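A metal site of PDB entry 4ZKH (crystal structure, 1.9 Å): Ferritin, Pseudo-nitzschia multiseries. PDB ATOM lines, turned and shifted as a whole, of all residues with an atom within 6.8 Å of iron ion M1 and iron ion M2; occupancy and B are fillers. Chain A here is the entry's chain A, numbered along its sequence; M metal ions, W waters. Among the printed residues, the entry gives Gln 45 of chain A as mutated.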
ATOM      1  N   GLN A  12      32.195 -12.244  12.417  1.00  0.00           N
ATOM      2  CA  GLN A  12      31.155 -11.325  11.832  1.00  0.00           C
ATOM      3  C   GLN A  12      31.838 -10.290  10.988  1.00  0.00           C
ATOM      4  O   GLN A  12      31.341  -9.919   9.930  1.00  0.00           O
ATOM      5  CB  GLN A  12      30.251 -10.697  12.874  1.00  0.00           C
ATOM      6  CG  GLN A  12      29.088  -9.905  12.264  1.00  0.00           C
ATOM      7  CD  GLN A  12      28.128 -10.873  11.571  1.00  0.00           C
ATOM      8  OE1 GLN A  12      27.987 -12.006  12.032  1.00  0.00           O
ATOM      9  NE2 GLN A  12      27.508 -10.463  10.448  1.00  0.00           N
ATOM     10  N   GLN A  15      32.601 -11.836   7.750  1.00  0.00           N
ATOM     11  CA  GLN A  15      31.361 -11.941   6.975  1.00  0.00           C
ATOM     12  C   GLN A  15      30.942 -10.638   6.310  1.00  0.00           C
ATOM     13  O   GLN A  15      30.555 -10.685   5.171  1.00  0.00           O
ATOM     14  CB  GLN A  15      30.240 -12.488   7.846  1.00  0.00           C
ATOM     15  CG  GLN A  15      28.945 -12.673   7.094  1.00  0.00           C
ATOM     16  CD  GLN A  15      29.006 -13.739   5.993  1.00  0.00           C
ATOM     17  OE1 GLN A  15      29.732 -14.734   6.112  1.00  0.00           O
ATOM     18  NE2 GLN A  15      28.252 -13.513   4.887  1.00  0.00           N
ATOM     19  N   GLU A  16      31.045  -9.507   7.005  1.00  0.00           N
ATOM     20  CA  GLU A  16      30.644  -8.236   6.426  1.00  0.00           C
ATOM     21  C   GLU A  16      31.611  -7.915   5.324  1.00  0.00           C
ATOM     22  O   GLU A  16      31.191  -7.493   4.240  1.00  0.00           O
ATOM     23  CB  GLU A  16      30.647  -7.147   7.494  1.00  0.00           C
ATOM     24  CG  GLU A  16      29.723  -7.393   8.630  1.00  0.00           C
ATOM     25  CD  GLU A  16      28.243  -7.335   8.258  1.00  0.00           C
ATOM     26  OE1 GLU A  16      27.968  -6.794   7.201  1.00  0.00           O
ATOM     27  OE2 GLU A  16      27.396  -7.894   9.048  1.00  0.00           O
ATOM     28  N   ALA A  19      30.881 -10.049   2.317  1.00  0.00           N
ATOM     29  CA  ALA A  19      29.766  -9.448   1.620  1.00  0.00           C
ATOM     30  C   ALA A  19      30.173  -8.243   0.814  1.00  0.00           C
ATOM     31  O   ALA A  19      29.733  -8.113  -0.354  1.00  0.00           O
ATOM     32  CB  ALA A  19      28.624  -9.139   2.615  1.00  0.00           C
ATOM     33  N   TYR A  23      29.506  -8.045  -3.238  1.00  0.00           N
ATOM     34  CA  TYR A  23      28.830  -6.880  -3.881  1.00  0.00           C
ATOM     35  C   TYR A  23      29.714  -6.258  -4.942  1.00  0.00           C
ATOM     36  O   TYR A  23      29.206  -5.877  -5.993  1.00  0.00           O
ATOM     37  CB  TYR A  23      28.367  -5.854  -2.809  1.00  0.00           C
ATOM     38  CG  TYR A  23      27.009  -6.129  -2.200  1.00  0.00           C
ATOM     39  CD1 TYR A  23      25.871  -5.941  -2.955  1.00  0.00           C
ATOM     40  CD2 TYR A  23      26.845  -6.442  -0.874  1.00  0.00           C
ATOM     41  CE1 TYR A  23      24.630  -6.135  -2.423  1.00  0.00           C
ATOM     42  CE2 TYR A  23      25.649  -6.679  -0.330  1.00  0.00           C
ATOM     43  CZ  TYR A  23      24.500  -6.458  -1.098  1.00  0.00           C
ATOM     44  OH  TYR A  23      23.258  -6.674  -0.587  1.00  0.00           O
ATOM     45  N   GLN A  45      26.188  -0.794  -2.123  1.00  0.00           N
ATOM     46  CA  GLN A  45      26.055  -1.821  -1.108  1.00  0.00           C
ATOM     47  C   GLN A  45      27.447  -2.400  -0.655  1.00  0.00           C
ATOM     48  O   GLN A  45      27.608  -2.743   0.491  1.00  0.00           O
ATOM     49  CB  GLN A  45      25.186  -2.961  -1.632  1.00  0.00           C
ATOM     50  CG  GLN A  45      23.711  -2.669  -1.506  1.00  0.00           C
ATOM     51  CD  GLN A  45      23.380  -2.496  -0.043  1.00  0.00           C
ATOM     52  OE1 GLN A  45      23.684  -3.354   0.802  1.00  0.00           O
ATOM     53  NE2 GLN A  45      22.885  -1.341   0.287  1.00  0.00           N
ATOM     54  N   GLU A  48      28.497  -0.054   1.921  1.00  0.00           N
ATOM     55  CA  GLU A  48      27.714  -0.220   3.135  1.00  0.00           C
ATOM     56  C   GLU A  48      28.185  -1.469   3.969  1.00  0.00           C
ATOM     57  O   GLU A  48      28.268  -1.398   5.183  1.00  0.00           O
ATOM     58  CB  GLU A  48      26.247  -0.316   2.792  1.00  0.00           C
ATOM     59  CG  GLU A  48      25.266  -0.620   3.914  1.00  0.00           C
ATOM     60  CD  GLU A  48      24.928   0.620   4.756  1.00  0.00           C
ATOM     61  OE1 GLU A  48      25.320   1.761   4.336  1.00  0.00           O
ATOM     62  OE2 GLU A  48      24.270   0.425   5.850  1.00  0.00           O
ATOM     63  N   GLU A  49      28.442  -2.607   3.321  1.00  0.00           N
ATOM     64  CA  GLU A  49      28.867  -3.766   4.065  1.00  0.00           C
ATOM     65  C   GLU A  49      30.188  -3.532   4.719  1.00  0.00           C
ATOM     66  O   GLU A  49      30.409  -3.996   5.878  1.00  0.00           O
ATOM     67  CB  GLU A  49      28.960  -4.988   3.115  1.00  0.00           C
ATOM     68  CG  GLU A  49      27.655  -5.360   2.524  1.00  0.00           C
ATOM     69  CD  GLU A  49      26.719  -5.977   3.502  1.00  0.00           C
ATOM     70  OE1 GLU A  49      27.024  -6.103   4.693  1.00  0.00           O
ATOM     71  OE2 GLU A  49      25.718  -6.466   3.037  1.00  0.00           O
ATOM     72  N   ARG A  50      31.097  -2.810   4.048  1.00  0.00           N
ATOM     73  CA  ARG A  50      32.360  -2.453   4.667  1.00  0.00           C
ATOM     74  C   ARG A  50      32.102  -1.588   5.887  1.00  0.00           C
ATOM     75  O   ARG A  50      32.740  -1.787   6.904  1.00  0.00           O
ATOM     76  CB  ARG A  50      33.321  -1.752   3.696  1.00  0.00           C
ATOM     77  CG  ARG A  50      34.618  -1.218   4.319  1.00  0.00           C
ATOM     78  CD  ARG A  50      35.783  -1.097   3.293  1.00  0.00           C
ATOM     79  NE  ARG A  50      37.105  -0.818   3.951  1.00  0.00           N
ATOM     80  CZ  ARG A  50      37.334   0.417   4.340  1.00  0.00           C
ATOM     81  NH1 ARG A  50      36.374   1.306   4.136  1.00  0.00           N
ATOM     82  NH2 ARG A  50      38.389   0.787   5.003  1.00  0.00           N
ATOM     83  N   HIS A  52      29.536  -1.815   7.770  1.00  0.00           N
ATOM     84  CA  HIS A  52      29.091  -2.670   8.859  1.00  0.00           C
ATOM     85  C   HIS A  52      30.284  -3.354   9.515  1.00  0.00           C
ATOM     86  O   HIS A  52      30.327  -3.440  10.712  1.00  0.00           O
ATOM     87  CB  HIS A  52      28.156  -3.783   8.424  1.00  0.00           C
ATOM     88  CG  HIS A  52      26.869  -3.268   7.822  1.00  0.00           C
ATOM     89  ND1 HIS A  52      26.065  -4.057   7.008  1.00  0.00           N
ATOM     90  CD2 HIS A  52      26.298  -2.031   7.844  1.00  0.00           C
ATOM     91  CE1 HIS A  52      25.030  -3.334   6.593  1.00  0.00           C
ATOM     92  NE2 HIS A  52      25.151  -2.103   7.065  1.00  0.00           N
ATOM     93  N   GLY A  53      31.207  -3.865   8.716  1.00  0.00           N
ATOM     94  CA  GLY A  53      32.411  -4.477   9.282  1.00  0.00           C
ATOM     95  C   GLY A  53      33.203  -3.535  10.149  1.00  0.00           C
ATOM     96  O   GLY A  53      33.657  -3.907  11.251  1.00  0.00           O
ATOM     97  N   LEU A  94      23.420 -14.106  -0.021  1.00  0.00           N
ATOM     98  CA  LEU A  94      24.456 -13.391   0.777  1.00  0.00           C
ATOM     99  C   LEU A  94      23.815 -12.649   1.957  1.00  0.00           C
ATOM    100  O   LEU A  94      24.261 -12.753   3.098  1.00  0.00           O
ATOM    101  CB  LEU A  94      25.154 -12.380  -0.115  1.00  0.00           C
ATOM    102  CG  LEU A  94      26.245 -11.523   0.533  1.00  0.00           C
ATOM    103  CD1 LEU A  94      27.405 -12.455   0.892  1.00  0.00           C
ATOM    104  CD2 LEU A  94      26.666 -10.409  -0.413  1.00  0.00           C
ATOM    105  N   GLU A  95      22.725 -11.903   1.719  1.00  0.00           N
ATOM    106  CA  GLU A  95      22.094 -11.186   2.792  1.00  0.00           C
ATOM    107  C   GLU A  95      21.485 -12.128   3.808  1.00  0.00           C
ATOM    108  O   GLU A  95      21.607 -11.885   5.015  1.00  0.00           O
ATOM    109  CB  GLU A  95      21.083 -10.137   2.340  1.00  0.00           C
ATOM    110  CG  GLU A  95      21.789  -9.044   1.589  1.00  0.00           C
ATOM    111  CD  GLU A  95      22.621  -8.103   2.476  1.00  0.00           C
ATOM    112  OE1 GLU A  95      22.732  -8.338   3.709  1.00  0.00           O
ATOM    113  OE2 GLU A  95      23.143  -7.145   1.850  1.00  0.00           O
ATOM    114  N   ASN A  98      24.267 -13.172   5.939  1.00  0.00           N
ATOM    115  CA  ASN A  98      24.644 -12.095   6.874  1.00  0.00           C
ATOM    116  C   ASN A  98      23.698 -12.155   8.092  1.00  0.00           C
ATOM    117  O   ASN A  98      24.122 -12.110   9.235  1.00  0.00           O
ATOM    118  CB  ASN A  98      24.584 -10.701   6.233  1.00  0.00           C
ATOM    119  CG  ASN A  98      25.726 -10.424   5.279  1.00  0.00           C
ATOM    120  OD1 ASN A  98      26.710 -11.187   5.192  1.00  0.00           O
ATOM    121  ND2 ASN A  98      25.605  -9.313   4.562  1.00  0.00           N
ATOM    122  N   LEU A 102      24.402 -12.965  12.167  1.00  0.00           N
ATOM    123  CA  LEU A 102      24.069 -12.027  13.239  1.00  0.00           C
ATOM    124  C   LEU A 102      23.191 -12.676  14.284  1.00  0.00           C
ATOM    125  O   LEU A 102      23.332 -12.403  15.450  1.00  0.00           O
ATOM    126  CB  LEU A 102      23.327 -10.783  12.701  1.00  0.00           C
ATOM    127  CG  LEU A 102      24.238  -9.855  11.922  1.00  0.00           C
ATOM    128  CD1 LEU A 102      23.405  -8.887  11.082  1.00  0.00           C
ATOM    129  CD2 LEU A 102      25.109  -9.013  12.837  1.00  0.00           C
ATOM    130  N   PHE A 124      21.352  -3.851  13.784  1.00  0.00           N
ATOM    131  CA  PHE A 124      21.790  -4.653  12.669  1.00  0.00           C
ATOM    132  C   PHE A 124      20.677  -5.674  12.355  1.00  0.00           C
ATOM    133  O   PHE A 124      20.473  -5.978  11.194  1.00  0.00           O
ATOM    134  CB  PHE A 124      23.130  -5.369  12.953  1.00  0.00           C
ATOM    135  CG  PHE A 124      24.287  -4.417  12.971  1.00  0.00           C
ATOM    136  CD1 PHE A 124      24.928  -4.054  11.782  1.00  0.00           C
ATOM    137  CD2 PHE A 124      24.706  -3.833  14.176  1.00  0.00           C
ATOM    138  CE1 PHE A 124      25.981  -3.155  11.803  1.00  0.00           C
ATOM    139  CE2 PHE A 124      25.764  -2.918  14.207  1.00  0.00           C
ATOM    140  CZ  PHE A 124      26.394  -2.551  12.996  1.00  0.00           C
ATOM    141  N   GLN A 127      18.120  -3.635  10.453  1.00  0.00           N
ATOM    142  CA  GLN A 127      18.656  -3.353   9.108  1.00  0.00           C
ATOM    143  C   GLN A 127      18.513  -4.624   8.200  1.00  0.00           C
ATOM    144  O   GLN A 127      18.184  -4.529   7.034  1.00  0.00           O
ATOM    145  CB  GLN A 127      20.115  -2.949   9.273  1.00  0.00           C
ATOM    146  CG  GLN A 127      20.888  -2.777   7.973  1.00  0.00           C
ATOM    147  CD  GLN A 127      20.642  -1.450   7.341  1.00  0.00           C
ATOM    148  OE1 GLN A 127      19.767  -0.660   7.799  1.00  0.00           O
ATOM    149  NE2 GLN A 127      21.378  -1.167   6.260  1.00  0.00           N
ATOM    150  N   GLN A 128      18.911  -5.766   8.682  1.00  0.00           N
ATOM    151  CA  GLN A 128      18.831  -6.992   7.828  1.00  0.00           C
ATOM    152  C   GLN A 128      17.403  -7.282   7.348  1.00  0.00           C
ATOM    153  O   GLN A 128      17.216  -7.761   6.252  1.00  0.00           O
ATOM    154  CB  GLN A 128      19.348  -8.193   8.555  1.00  0.00           C
ATOM    155  CG  GLN A 128      20.851  -8.238   8.667  1.00  0.00           C
ATOM    156  CD  GLN A 128      21.579  -7.901   7.355  1.00  0.00           C
ATOM    157  OE1 GLN A 128      22.187  -6.807   7.169  1.00  0.00           O
ATOM    158  NE2 GLN A 128      21.528  -8.853   6.425  1.00  0.00           N
ATOM    159  N   GLU A 131      16.907  -4.951   4.559  1.00  0.00           N
ATOM    160  CA  GLU A 131      17.710  -5.327   3.405  1.00  0.00           C
ATOM    161  C   GLU A 131      17.201  -6.590   2.675  1.00  0.00           C
ATOM    162  O   GLU A 131      17.219  -6.617   1.413  1.00  0.00           O
ATOM    163  CB  GLU A 131      19.193  -5.497   3.784  1.00  0.00           C
ATOM    164  CG  GLU A 131      19.908  -4.160   4.051  1.00  0.00           C
ATOM    165  CD  GLU A 131      21.383  -4.369   4.357  1.00  0.00           C
ATOM    166  OE1 GLU A 131      21.829  -5.497   4.088  1.00  0.00           O
ATOM    167  OE2 GLU A 131      22.089  -3.468   4.907  1.00  0.00           O
HETATM  168 FE    FE M   1      23.862  -6.125   3.733  1.00  0.00          FE
HETATM  169 FE    FE M   2      26.064  -6.379   6.436  1.00  0.00          FE
HETATM  170  O   HOH W   1      24.338  -4.041   3.106  1.00  0.00           O
HETATM  171  O   HOH W   2      25.124  -7.001   8.125  1.00  0.00           O
HETATM  172  O   HOH W   3      24.118  -6.504   5.488  1.00  0.00           O
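The side-chain carboxylate (OE2) of Glu 49 sits close to the side-chain amide nitrogen (ND2) of Asn 98 (3.2 Å).
OE2 of Glu 16 sits at hydrogen-bond distance from NE2 of Gln 12 (2.9 Å).
The side-chain carboxylate of Glu 131 lies close to the side-chain amide oxygen of Gln 128 (3.4 Å).
OE2 of Glu 131 lies within hydrogen-bond range of NE2 of Gln 127 (2.8 Å).
OE1 of Glu 95 lies close to ND2 of Asn 98 (3.2 Å).
The side-chain carboxylate (OE2) of Glu 95 sits close to the side-chain hydroxyl (OH) of Tyr 23, 2.5 Å away.
OE2 of Glu 48 sits at hydrogen-bond distance from NE2 of His 52 (2.9 Å).
NE2 of Gln 15 lies within hydrogen-bond range of OD1 of Asn 98, 2.8 Å away.
Iron ion M1 is bound by water W3 (1.8 Å), OE2 of Glu 49 (2.0 Å), OE1 of Glu 131 (2.2 Å), water W1 (2.2 Å), OE2 of Glu 95 (2.3 Å) and OE1 of Glu 95 (2.5 Å).
Iron ion M1 has six donor atoms within binding distance.
ND2 of Asn 98 touches iron ion M2 (3.5 Å).
Gln 128 touches iron ion M2.
Of the 19 residues printed, 5 come within 4 Å of iron ion M2.
ND2 of Asn 98 touches iron ion M1, 3.7 Å away.
OE1 of Gln 128 touches iron ion M1, 3.9 Å away.
Five residues have an atom within 4 Å of iron ion M1: Glu 49, Glu 95, Asn 98, Gln 128 and Glu 131.
Water W1 lies within hydrogen-bond range of OE1 of Gln 45 and OE2 of Glu 131.
Water W3 lies within hydrogen-bond range of OE1 of Gln 128 and ND2 of Asn 98.
Water W2 bridges the side-chain carboxylate of Glu 16 (2.6 Å) and the side-chain amide oxygen of Gln 128 (3.1 Å).
Iron ion M2 is bound by OE1 of Glu 49, water W2, OE1 of Glu 16, water W3 and ND1 of His 52.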
